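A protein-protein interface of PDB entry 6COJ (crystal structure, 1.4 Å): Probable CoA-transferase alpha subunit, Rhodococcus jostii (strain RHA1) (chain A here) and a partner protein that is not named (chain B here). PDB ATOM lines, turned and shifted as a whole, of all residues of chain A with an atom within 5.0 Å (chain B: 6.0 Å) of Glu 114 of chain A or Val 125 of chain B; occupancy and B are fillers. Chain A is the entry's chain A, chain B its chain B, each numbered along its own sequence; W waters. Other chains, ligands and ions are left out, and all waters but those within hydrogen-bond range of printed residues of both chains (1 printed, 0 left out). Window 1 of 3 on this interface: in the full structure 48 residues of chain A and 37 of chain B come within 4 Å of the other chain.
O of Gly 87 of chain A sits at hydrogen-bond distance from N of Arg 126 of chain B (3.1 Å). The guanidinium group (NH1) of Arg 105 of chain A lies within hydrogen-bond range of the backbone carbonyl oxygen (O) of Leu 115 of chain B, 2.8 Å away. The side-chain amide oxygen of Gln 121 of chain B lies within hydrogen-bond range of the guanidinium group of Arg 105 of chain A (2.8 Å). The side-chain hydroxyl of Ser 110 of chain B lies within hydrogen-bond range of the side-chain carboxylate of Glu 114 of chain A (2.6 Å). The side-chain carboxylate (OE2) of Glu 114 of chain A is in hydrogen-bond range of the backbone NH (N) of Val 125 of chain B. The side-chain carboxylate (OD1) of Asp 116 of chain A sits close to the backbone carbonyl oxygen (O) of Arg 126 of chain B (3.4 Å). OD1 of Asp 116 of chain A lies close to O of Gly 127 of chain B (3.3 Å).
OE1 of Glu 114 of chain A sits at hydrogen-bond distance from OH of Tyr 86 of chain A (2.7 Å). The backbone carbonyl oxygen (O) of Tyr 86 of chain A sits at hydrogen-bond distance from the backbone NH (N) of Met 115 of chain A, 3.0 Å away. The guanidinium group of Arg 113 of chain A is in hydrogen-bond range of the backbone carbonyl oxygen of Phe 147 of chain A, at 3.5 Å. The backbone carbonyl oxygen (O) of Ser 110 of chain B sits at hydrogen-bond distance from the side-chain amide nitrogen (NE2) of Gln 121 of chain B (3.3 Å). The backbone carbonyl oxygen (O) of Ser 110 of chain B sits at hydrogen-bond distance from the backbone NH (N) of Phe 123 of chain B, at 3.5 Å. The backbone carbonyl oxygen (O) of Ser 110 of chain B lies within hydrogen-bond range of the backbone NH (N) of Gly 124 of chain B (3.2 Å).
Among the printed residues, pairs that only touch across the chains: Glu 114 of chain A with Gly 124 of chain B (3.1 Å), Met 115 of chain A with Val 125 of chain B (3.2 Å), Asp 116 of chain A with Val 125 of chain B (3.7 Å), Asp 116 of chain A with Pro 129 of chain B (3.4 Å), Val 144 of chain A with Pro 129 of chain B (3.99 Å) and Phe 147 of chain A with Leu 115 of chain B (3.5 Å).
Printed residues of chain B within 4 Å of Glu 114 of chain A: Ser 110 (2.6 Å), Gly 124 (3.1 Å) and Val 125 (2.9 Å). Val 125 of chain B touches just these residues of chain A: Glu 114 (2.9 Å), Met 115 (3.2 Å) and Asp 116 (3.7 Å). Of the printed residues of chain B, Phe 147 of chain A touches Leu 115. Of the printed residues of chain B, Arg 105 of chain A touches Leu 115 and Gln 121. Printed residues of chain B within 4 Å of Val 144 of chain A: Pro 129. The nearest residue of chain B that does not touch Glu 114 of chain A is Gln 121 of chain B (4.8 Å). The nearest residue of chain A that does not touch Val 125 of chain B is Gly 87 of chain A (4.2 Å). The nearest printed residue of chain A that does not touch Gly 124 of chain B is Gly 87 of chain A (4.7 Å).
Of the 15 printed residues of chain B, 8 touch a printed residue of chain A. Hydrophobic or aromatic side chains of chain B that line the printed part of chain A: Leu 115, Val 125 and Pro 129. Hydrophobic or aromatic side chains of chain A that line the printed part of chain B: Val 144 and Phe 147. Among the printed residues, 13 pairs touch across the chains. Among the printed residues, no Asp or Glu carboxylate lies within 4 Å of a Lys or Arg side-chain nitrogen of the other chain.
Water W1 lies within hydrogen-bond range of the side-chain carboxylate of Glu 114 of chain A (2.7 Å), the side-chain hydroxyl of Ser 110 of chain B (2.8 Å), the guanidinium group of Arg 105 of chain A (2.9 Å) and the side-chain amide nitrogen of Gln 121 of chain B (3.0 Å).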
ATOM      1  N   ALA A  84     -13.412  25.903 -12.271  1.00  0.00           N
ATOM      2  CA  ALA A  84     -13.104  27.256 -12.716  1.00  0.00           C
ATOM      3  C   ALA A  84     -11.885  27.245 -13.621  1.00  0.00           C
ATOM      4  O   ALA A  84     -10.853  26.669 -13.268  1.00  0.00           O
ATOM      5  CB  ALA A  84     -12.884  28.199 -11.522  1.00  0.00           C
ATOM      6  N   TYR A  86      -9.412  30.005 -15.316  1.00  0.00           N
ATOM      7  CA  TYR A  86      -9.123  31.429 -15.131  1.00  0.00           C
ATOM      8  C   TYR A  86      -7.638  31.682 -15.319  1.00  0.00           C
ATOM      9  O   TYR A  86      -6.809  30.793 -15.095  1.00  0.00           O
ATOM     10  CB  TYR A  86      -9.560  31.918 -13.730  1.00  0.00           C
ATOM     11  CG  TYR A  86      -8.935  31.106 -12.608  1.00  0.00           C
ATOM     12  CD1 TYR A  86      -9.551  29.957 -12.130  1.00  0.00           C
ATOM     13  CD2 TYR A  86      -7.701  31.460 -12.072  1.00  0.00           C
ATOM     14  CE1 TYR A  86      -8.970  29.194 -11.127  1.00  0.00           C
ATOM     15  CE2 TYR A  86      -7.105  30.694 -11.083  1.00  0.00           C
ATOM     16  CZ  TYR A  86      -7.737  29.564 -10.628  1.00  0.00           C
ATOM     17  OH  TYR A  86      -7.159  28.802  -9.642  1.00  0.00           O
ATOM     18  N   GLY A  87      -7.315  32.920 -15.701  1.00  0.00           N
ATOM     19  CA  GLY A  87      -5.935  33.341 -15.841  1.00  0.00           C
ATOM     20  C   GLY A  87      -5.409  33.963 -14.568  1.00  0.00           C
ATOM     21  O   GLY A  87      -4.197  34.014 -14.341  1.00  0.00           O
ATOM     22  N   ARG A 105     -10.902  27.918  -2.456  1.00  0.00           N
ATOM     23  CA  ARG A 105      -9.664  27.225  -2.806  1.00  0.00           C
ATOM     24  C   ARG A 105      -9.081  26.480  -1.608  1.00  0.00           C
ATOM     25  O   ARG A 105      -8.734  25.294  -1.707  1.00  0.00           O
ATOM     26  CB  ARG A 105      -8.661  28.240  -3.351  1.00  0.00           C
ATOM     27  CG  ARG A 105      -9.051  28.797  -4.724  1.00  0.00           C
ATOM     28  CD  ARG A 105      -8.617  27.845  -5.829  1.00  0.00           C
ATOM     29  NE  ARG A 105      -7.170  27.859  -5.981  1.00  0.00           N
ATOM     30  CZ  ARG A 105      -6.416  26.787  -6.199  1.00  0.00           C
ATOM     31  NH1 ARG A 105      -6.952  25.567  -6.253  1.00  0.00           N
ATOM     32  NH2 ARG A 105      -5.107  26.933  -6.348  1.00  0.00           N
ATOM     33  N   VAL A 112      -9.813  23.439 -10.213  1.00  0.00           N
ATOM     34  CA  VAL A 112      -9.304  24.572 -10.983  1.00  0.00           C
ATOM     35  C   VAL A 112      -8.555  24.104 -12.220  1.00  0.00           C
ATOM     36  O   VAL A 112      -7.786  23.134 -12.179  1.00  0.00           O
ATOM     37  CB  VAL A 112      -8.479  25.590 -10.164  1.00  0.00           C
ATOM     38  CG1 VAL A 112      -9.306  26.147  -8.997  1.00  0.00           C
ATOM     39  CG2 VAL A 112      -7.184  24.978  -9.668  1.00  0.00           C
ATOM     40  N   ARG A 113      -8.796  24.810 -13.326  1.00  0.00           N
ATOM     41  CA  ARG A 113      -7.935  24.737 -14.500  1.00  0.00           C
ATOM     42  C   ARG A 113      -7.309  26.113 -14.687  1.00  0.00           C
ATOM     43  O   ARG A 113      -7.578  26.831 -15.663  1.00  0.00           O
ATOM     44  CB  ARG A 113      -8.712  24.261 -15.721  1.00  0.00           C
ATOM     45  CG  ARG A 113      -9.275  22.853 -15.569  1.00  0.00           C
ATOM     46  CD  ARG A 113      -8.175  21.783 -15.420  1.00  0.00           C
ATOM     47  NE  ARG A 113      -8.757  20.456 -15.255  1.00  0.00           N
ATOM     48  CZ  ARG A 113      -9.029  19.903 -14.079  1.00  0.00           C
ATOM     49  NH1 ARG A 113      -8.740  20.552 -12.958  1.00  0.00           N
ATOM     50  NH2 ARG A 113      -9.575  18.696 -14.033  1.00  0.00           N
ATOM     51  N   GLU A 114      -6.486  26.480 -13.711  1.00  0.00           N
ATOM     52  CA  GLU A 114      -5.740  27.724 -13.736  1.00  0.00           C
ATOM     53  C   GLU A 114      -4.784  27.707 -14.922  1.00  0.00           C
ATOM     54  O   GLU A 114      -4.221  26.663 -15.272  1.00  0.00           O
ATOM     55  CB  GLU A 114      -4.975  27.829 -12.411  1.00  0.00           C
ATOM     56  CG  GLU A 114      -4.196  29.110 -12.225  1.00  0.00           C
ATOM     57  CD  GLU A 114      -3.692  29.267 -10.807  1.00  0.00           C
ATOM     58  OE1 GLU A 114      -4.475  29.023  -9.871  1.00  0.00           O
ATOM     59  OE2 GLU A 114      -2.509  29.620 -10.629  1.00  0.00           O
ATOM     60  N   MET A 115      -4.617  28.861 -15.560  1.00  0.00           N
ATOM     61  CA  MET A 115      -3.815  28.909 -16.774  1.00  0.00           C
ATOM     62  C   MET A 115      -3.178  30.279 -16.911  1.00  0.00           C
ATOM     63  O   MET A 115      -3.583  31.244 -16.259  1.00  0.00           O
ATOM     64  CB  MET A 115      -4.667  28.585 -18.006  1.00  0.00           C
ATOM     65  CG  MET A 115      -5.689  29.660 -18.347  1.00  0.00           C
ATOM     66  SD  MET A 115      -6.792  29.166 -19.693  1.00  0.00           S
ATOM     67  CE  MET A 115      -8.238  28.642 -18.759  1.00  0.00           C
ATOM     68  N   ASP A 116      -2.164  30.364 -17.771  1.00  0.00           N
ATOM     69  CA  ASP A 116      -1.592  31.670 -18.077  1.00  0.00           C
ATOM     70  C   ASP A 116      -2.675  32.593 -18.636  1.00  0.00           C
ATOM     71  O   ASP A 116      -3.583  32.153 -19.344  1.00  0.00           O
ATOM     72  CB  ASP A 116      -0.452  31.527 -19.084  1.00  0.00           C
ATOM     73  CG  ASP A 116       0.066  32.865 -19.553  1.00  0.00           C
ATOM     74  OD1 ASP A 116       0.931  33.451 -18.862  1.00  0.00           O
ATOM     75  OD2 ASP A 116      -0.410  33.338 -20.604  1.00  0.00           O
ATOM     76  N   VAL A 144       1.121  25.150 -14.940  1.00  0.00           N
ATOM     77  CA  VAL A 144      -0.114  25.037 -15.705  1.00  0.00           C
ATOM     78  C   VAL A 144      -0.329  23.594 -16.160  1.00  0.00           C
ATOM     79  O   VAL A 144      -1.454  23.080 -16.136  1.00  0.00           O
ATOM     80  CB  VAL A 144      -0.118  26.034 -16.878  1.00  0.00           C
ATOM     81  CG1 VAL A 144      -1.360  25.828 -17.735  1.00  0.00           C
ATOM     82  CG2 VAL A 144      -0.067  27.455 -16.347  1.00  0.00           C
ATOM     83  N   PHE A 147      -1.857  21.696 -13.196  1.00  0.00           N
ATOM     84  CA  PHE A 147      -3.247  22.062 -12.940  1.00  0.00           C
ATOM     85  C   PHE A 147      -4.195  21.284 -13.847  1.00  0.00           C
ATOM     86  O   PHE A 147      -5.295  20.901 -13.427  1.00  0.00           O
ATOM     87  CB  PHE A 147      -3.460  23.561 -13.172  1.00  0.00           C
ATOM     88  CG  PHE A 147      -3.077  24.437 -12.012  1.00  0.00           C
ATOM     89  CD1 PHE A 147      -3.752  24.352 -10.798  1.00  0.00           C
ATOM     90  CD2 PHE A 147      -2.081  25.392 -12.151  1.00  0.00           C
ATOM     91  CE1 PHE A 147      -3.406  25.174  -9.745  1.00  0.00           C
ATOM     92  CE2 PHE A 147      -1.733  26.223 -11.108  1.00  0.00           C
ATOM     93  CZ  PHE A 147      -2.401  26.118  -9.890  1.00  0.00           C
ATOM     94  N   TRP A 148      -3.794  21.050 -15.097  1.00  0.00           N
ATOM     95  CA  TRP A 148      -4.679  20.462 -16.095  1.00  0.00           C
ATOM     96  C   TRP A 148      -4.470  18.977 -16.307  1.00  0.00           C
ATOM     97  O   TRP A 148      -5.402  18.297 -16.753  1.00  0.00           O
ATOM     98  CB  TRP A 148      -4.457  21.125 -17.449  1.00  0.00           C
ATOM     99  CG  TRP A 148      -4.935  22.520 -17.581  1.00  0.00           C
ATOM    100  CD1 TRP A 148      -4.477  23.618 -16.908  1.00  0.00           C
ATOM    101  CD2 TRP A 148      -5.938  22.990 -18.492  1.00  0.00           C
ATOM    102  NE1 TRP A 148      -5.144  24.742 -17.340  1.00  0.00           N
ATOM    103  CE2 TRP A 148      -6.046  24.380 -18.309  1.00  0.00           C
ATOM    104  CE3 TRP A 148      -6.768  22.363 -19.432  1.00  0.00           C
ATOM    105  CZ2 TRP A 148      -6.937  25.159 -19.045  1.00  0.00           C
ATOM    106  CZ3 TRP A 148      -7.665  23.136 -20.148  1.00  0.00           C
ATOM    107  CH2 TRP A 148      -7.736  24.521 -19.953  1.00  0.00           C
ATOM    108  N   LEU B 109       3.869  33.115  -7.809  1.00  0.00           N
ATOM    109  CA  LEU B 109       2.958  34.133  -7.294  1.00  0.00           C
ATOM    110  C   LEU B 109       1.515  33.636  -7.301  1.00  0.00           C
ATOM    111  O   LEU B 109       0.580  34.437  -7.160  1.00  0.00           O
ATOM    112  CB  LEU B 109       3.097  35.463  -8.046  1.00  0.00           C
ATOM    113  CG  LEU B 109       3.178  35.414  -9.573  1.00  0.00           C
ATOM    114  CD1 LEU B 109       1.940  34.779 -10.208  1.00  0.00           C
ATOM    115  CD2 LEU B 109       3.409  36.824 -10.137  1.00  0.00           C
ATOM    116  N   SER B 110       1.322  32.322  -7.431  1.00  0.00           N
ATOM    117  CA  SER B 110      -0.006  31.733  -7.572  1.00  0.00           C
ATOM    118  C   SER B 110      -0.669  31.447  -6.228  1.00  0.00           C
ATOM    119  O   SER B 110      -1.735  31.995  -5.926  1.00  0.00           O
ATOM    120  CB  SER B 110       0.084  30.444  -8.392  1.00  0.00           C
ATOM    121  OG  SER B 110      -1.147  29.748  -8.373  1.00  0.00           O
ATOM    122  N   ALA B 111      -0.055  30.586  -5.416  1.00  0.00           N
ATOM    123  CA  ALA B 111      -0.634  30.124  -4.158  1.00  0.00           C
ATOM    124  C   ALA B 111       0.422  29.299  -3.444  1.00  0.00           C
ATOM    125  O   ALA B 111       1.418  28.885  -4.047  1.00  0.00           O
ATOM    126  CB  ALA B 111      -1.880  29.265  -4.395  1.00  0.00           C
ATOM    127  N   LEU B 115      -1.954  22.149  -5.285  1.00  0.00           N
ATOM    128  CA  LEU B 115      -2.514  22.920  -6.390  1.00  0.00           C
ATOM    129  C   LEU B 115      -4.030  23.008  -6.317  1.00  0.00           C
ATOM    130  O   LEU B 115      -4.601  24.050  -6.654  1.00  0.00           O
ATOM    131  CB  LEU B 115      -2.089  22.307  -7.727  1.00  0.00           C
ATOM    132  CG  LEU B 115      -0.776  22.799  -8.338  1.00  0.00           C
ATOM    133  CD1 LEU B 115       0.406  22.505  -7.428  1.00  0.00           C
ATOM    134  CD2 LEU B 115      -0.563  22.186  -9.722  1.00  0.00           C
ATOM    135  N   GLN B 121      -4.096  31.395  -0.795  1.00  0.00           N
ATOM    136  CA  GLN B 121      -4.368  31.760  -2.178  1.00  0.00           C
ATOM    137  C   GLN B 121      -3.806  33.141  -2.477  1.00  0.00           C
ATOM    138  O   GLN B 121      -4.036  34.091  -1.723  1.00  0.00           O
ATOM    139  CB  GLN B 121      -5.873  31.769  -2.432  1.00  0.00           C
ATOM    140  CG  GLN B 121      -6.248  32.133  -3.852  1.00  0.00           C
ATOM    141  CD  GLN B 121      -5.720  31.116  -4.832  1.00  0.00           C
ATOM    142  OE1 GLN B 121      -5.886  29.911  -4.632  1.00  0.00           O
ATOM    143  NE2 GLN B 121      -5.058  31.586  -5.888  1.00  0.00           N
ATOM    144  N   PHE B 123      -2.716  35.261  -6.464  1.00  0.00           N
ATOM    145  CA  PHE B 123      -3.371  35.713  -7.686  1.00  0.00           C
ATOM    146  C   PHE B 123      -3.703  34.597  -8.657  1.00  0.00           C
ATOM    147  O   PHE B 123      -4.466  34.838  -9.603  1.00  0.00           O
ATOM    148  CB  PHE B 123      -2.453  36.667  -8.450  1.00  0.00           C
ATOM    149  CG  PHE B 123      -2.332  38.018  -7.836  1.00  0.00           C
ATOM    150  CD1 PHE B 123      -3.426  38.855  -7.748  1.00  0.00           C
ATOM    151  CD2 PHE B 123      -1.100  38.468  -7.375  1.00  0.00           C
ATOM    152  CE1 PHE B 123      -3.313  40.123  -7.193  1.00  0.00           C
ATOM    153  CE2 PHE B 123      -0.976  39.729  -6.826  1.00  0.00           C
ATOM    154  CZ  PHE B 123      -2.080  40.560  -6.747  1.00  0.00           C
ATOM    155  N   GLY B 124      -3.128  33.413  -8.484  1.00  0.00           N
ATOM    156  CA  GLY B 124      -2.979  32.504  -9.596  1.00  0.00           C
ATOM    157  C   GLY B 124      -1.805  32.949 -10.448  1.00  0.00           C
ATOM    158  O   GLY B 124      -1.163  33.969 -10.194  1.00  0.00           O
ATOM    159  N   VAL B 125      -1.544  32.176 -11.508  1.00  0.00           N
ATOM    160  CA  VAL B 125      -0.302  32.352 -12.267  1.00  0.00           C
ATOM    161  C   VAL B 125      -0.224  33.671 -13.030  1.00  0.00           C
ATOM    162  O   VAL B 125       0.883  34.089 -13.398  1.00  0.00           O
ATOM    163  CB  VAL B 125      -0.006  31.183 -13.228  1.00  0.00           C
ATOM    164  CG1 VAL B 125       0.166  29.879 -12.472  1.00  0.00           C
ATOM    165  CG2 VAL B 125      -1.074  31.083 -14.321  1.00  0.00           C
ATOM    166  N   ARG B 126      -1.353  34.339 -13.278  1.00  0.00           N
ATOM    167  CA  ARG B 126      -1.360  35.576 -14.061  1.00  0.00           C
ATOM    168  C   ARG B 126      -0.661  35.381 -15.406  1.00  0.00           C
ATOM    169  O   ARG B 126      -0.862  34.354 -16.057  1.00  0.00           O
ATOM    170  CB  ARG B 126      -0.754  36.740 -13.259  1.00  0.00           C
ATOM    171  CG  ARG B 126      -1.413  36.949 -11.876  1.00  0.00           C
ATOM    172  CD  ARG B 126      -1.626  38.426 -11.583  1.00  0.00           C
ATOM    173  NE  ARG B 126      -2.767  38.945 -12.341  1.00  0.00           N
ATOM    174  CZ  ARG B 126      -3.425  40.064 -12.052  1.00  0.00           C
ATOM    175  NH1 ARG B 126      -3.066  40.809 -11.008  1.00  0.00           N
ATOM    176  NH2 ARG B 126      -4.461  40.426 -12.797  1.00  0.00           N
ATOM    177  N   GLY B 127       0.170  36.340 -15.812  1.00  0.00           N
ATOM    178  CA  GLY B 127       0.954  36.212 -17.025  1.00  0.00           C
ATOM    179  C   GLY B 127       2.340  35.640 -16.832  1.00  0.00           C
ATOM    180  O   GLY B 127       3.118  35.635 -17.792  1.00  0.00           O
ATOM    181  N   ALA B 128       2.682  35.157 -15.638  1.00  0.00           N
ATOM    182  CA  ALA B 128       4.045  34.680 -15.405  1.00  0.00           C
ATOM    183  C   ALA B 128       4.479  33.550 -16.337  1.00  0.00           C
ATOM    184  O   ALA B 128       5.631  33.594 -16.813  1.00  0.00           O
ATOM    185  CB  ALA B 128       4.255  34.342 -13.921  1.00  0.00           C
ATOM    186  N   PRO B 129       3.664  32.527 -16.628  1.00  0.00           N
ATOM    187  CA  PRO B 129       4.141  31.485 -17.556  1.00  0.00           C
ATOM    188  C   PRO B 129       4.439  32.031 -18.944  1.00  0.00           C
ATOM    189  O   PRO B 129       5.500  31.734 -19.533  1.00  0.00           O
ATOM    190  CB  PRO B 129       3.001  30.450 -17.545  1.00  0.00           C
ATOM    191  CG  PRO B 129       2.220  30.722 -16.266  1.00  0.00           C
ATOM    192  CD  PRO B 129       2.342  32.193 -16.045  1.00  0.00           C
ATOM    193  N   ILE B 155       4.358  26.313  -6.347  1.00  0.00           N
ATOM    194  CA  ILE B 155       3.707  26.286  -7.651  1.00  0.00           C
ATOM    195  C   ILE B 155       4.591  27.052  -8.620  1.00  0.00           C
ATOM    196  O   ILE B 155       5.003  28.177  -8.327  1.00  0.00           O
ATOM    197  CB  ILE B 155       2.298  26.913  -7.589  1.00  0.00           C
ATOM    198  CG1 ILE B 155       1.402  26.140  -6.614  1.00  0.00           C
ATOM    199  CG2 ILE B 155       1.664  26.957  -8.967  1.00  0.00           C
ATOM    200  CD1 ILE B 155       0.046  26.797  -6.347  1.00  0.00           C
ATOM    201  N   VAL B 156       4.906  26.441  -9.762  1.00  0.00           N
ATOM    202  CA  VAL B 156       5.783  27.065 -10.754  1.00  0.00           C
ATOM    203  C   VAL B 156       4.906  27.936 -11.652  1.00  0.00           C
ATOM    204  O   VAL B 156       4.305  27.470 -12.620  1.00  0.00           O
ATOM    205  CB  VAL B 156       6.581  26.030 -11.544  1.00  0.00           C
ATOM    206  CG1 VAL B 156       7.431  26.715 -12.613  1.00  0.00           C
ATOM    207  CG2 VAL B 156       7.462  25.211 -10.614  1.00  0.00           C
ATOM    208  N   SER B 157       4.812  29.220 -11.310  1.00  0.00           N
ATOM    209  CA  SER B 157       4.176  30.176 -12.214  1.00  0.00           C
ATOM    210  C   SER B 157       5.172  30.827 -13.173  1.00  0.00           C
ATOM    211  O   SER B 157       4.824  31.118 -14.324  1.00  0.00           O
ATOM    212  CB  SER B 157       3.379  31.227 -11.431  1.00  0.00           C
ATOM    213  OG  SER B 157       4.191  31.971 -10.536  1.00  0.00           O
HETATM  214  O   HOH W   1      -3.750  29.348  -7.340  1.00  0.00           O
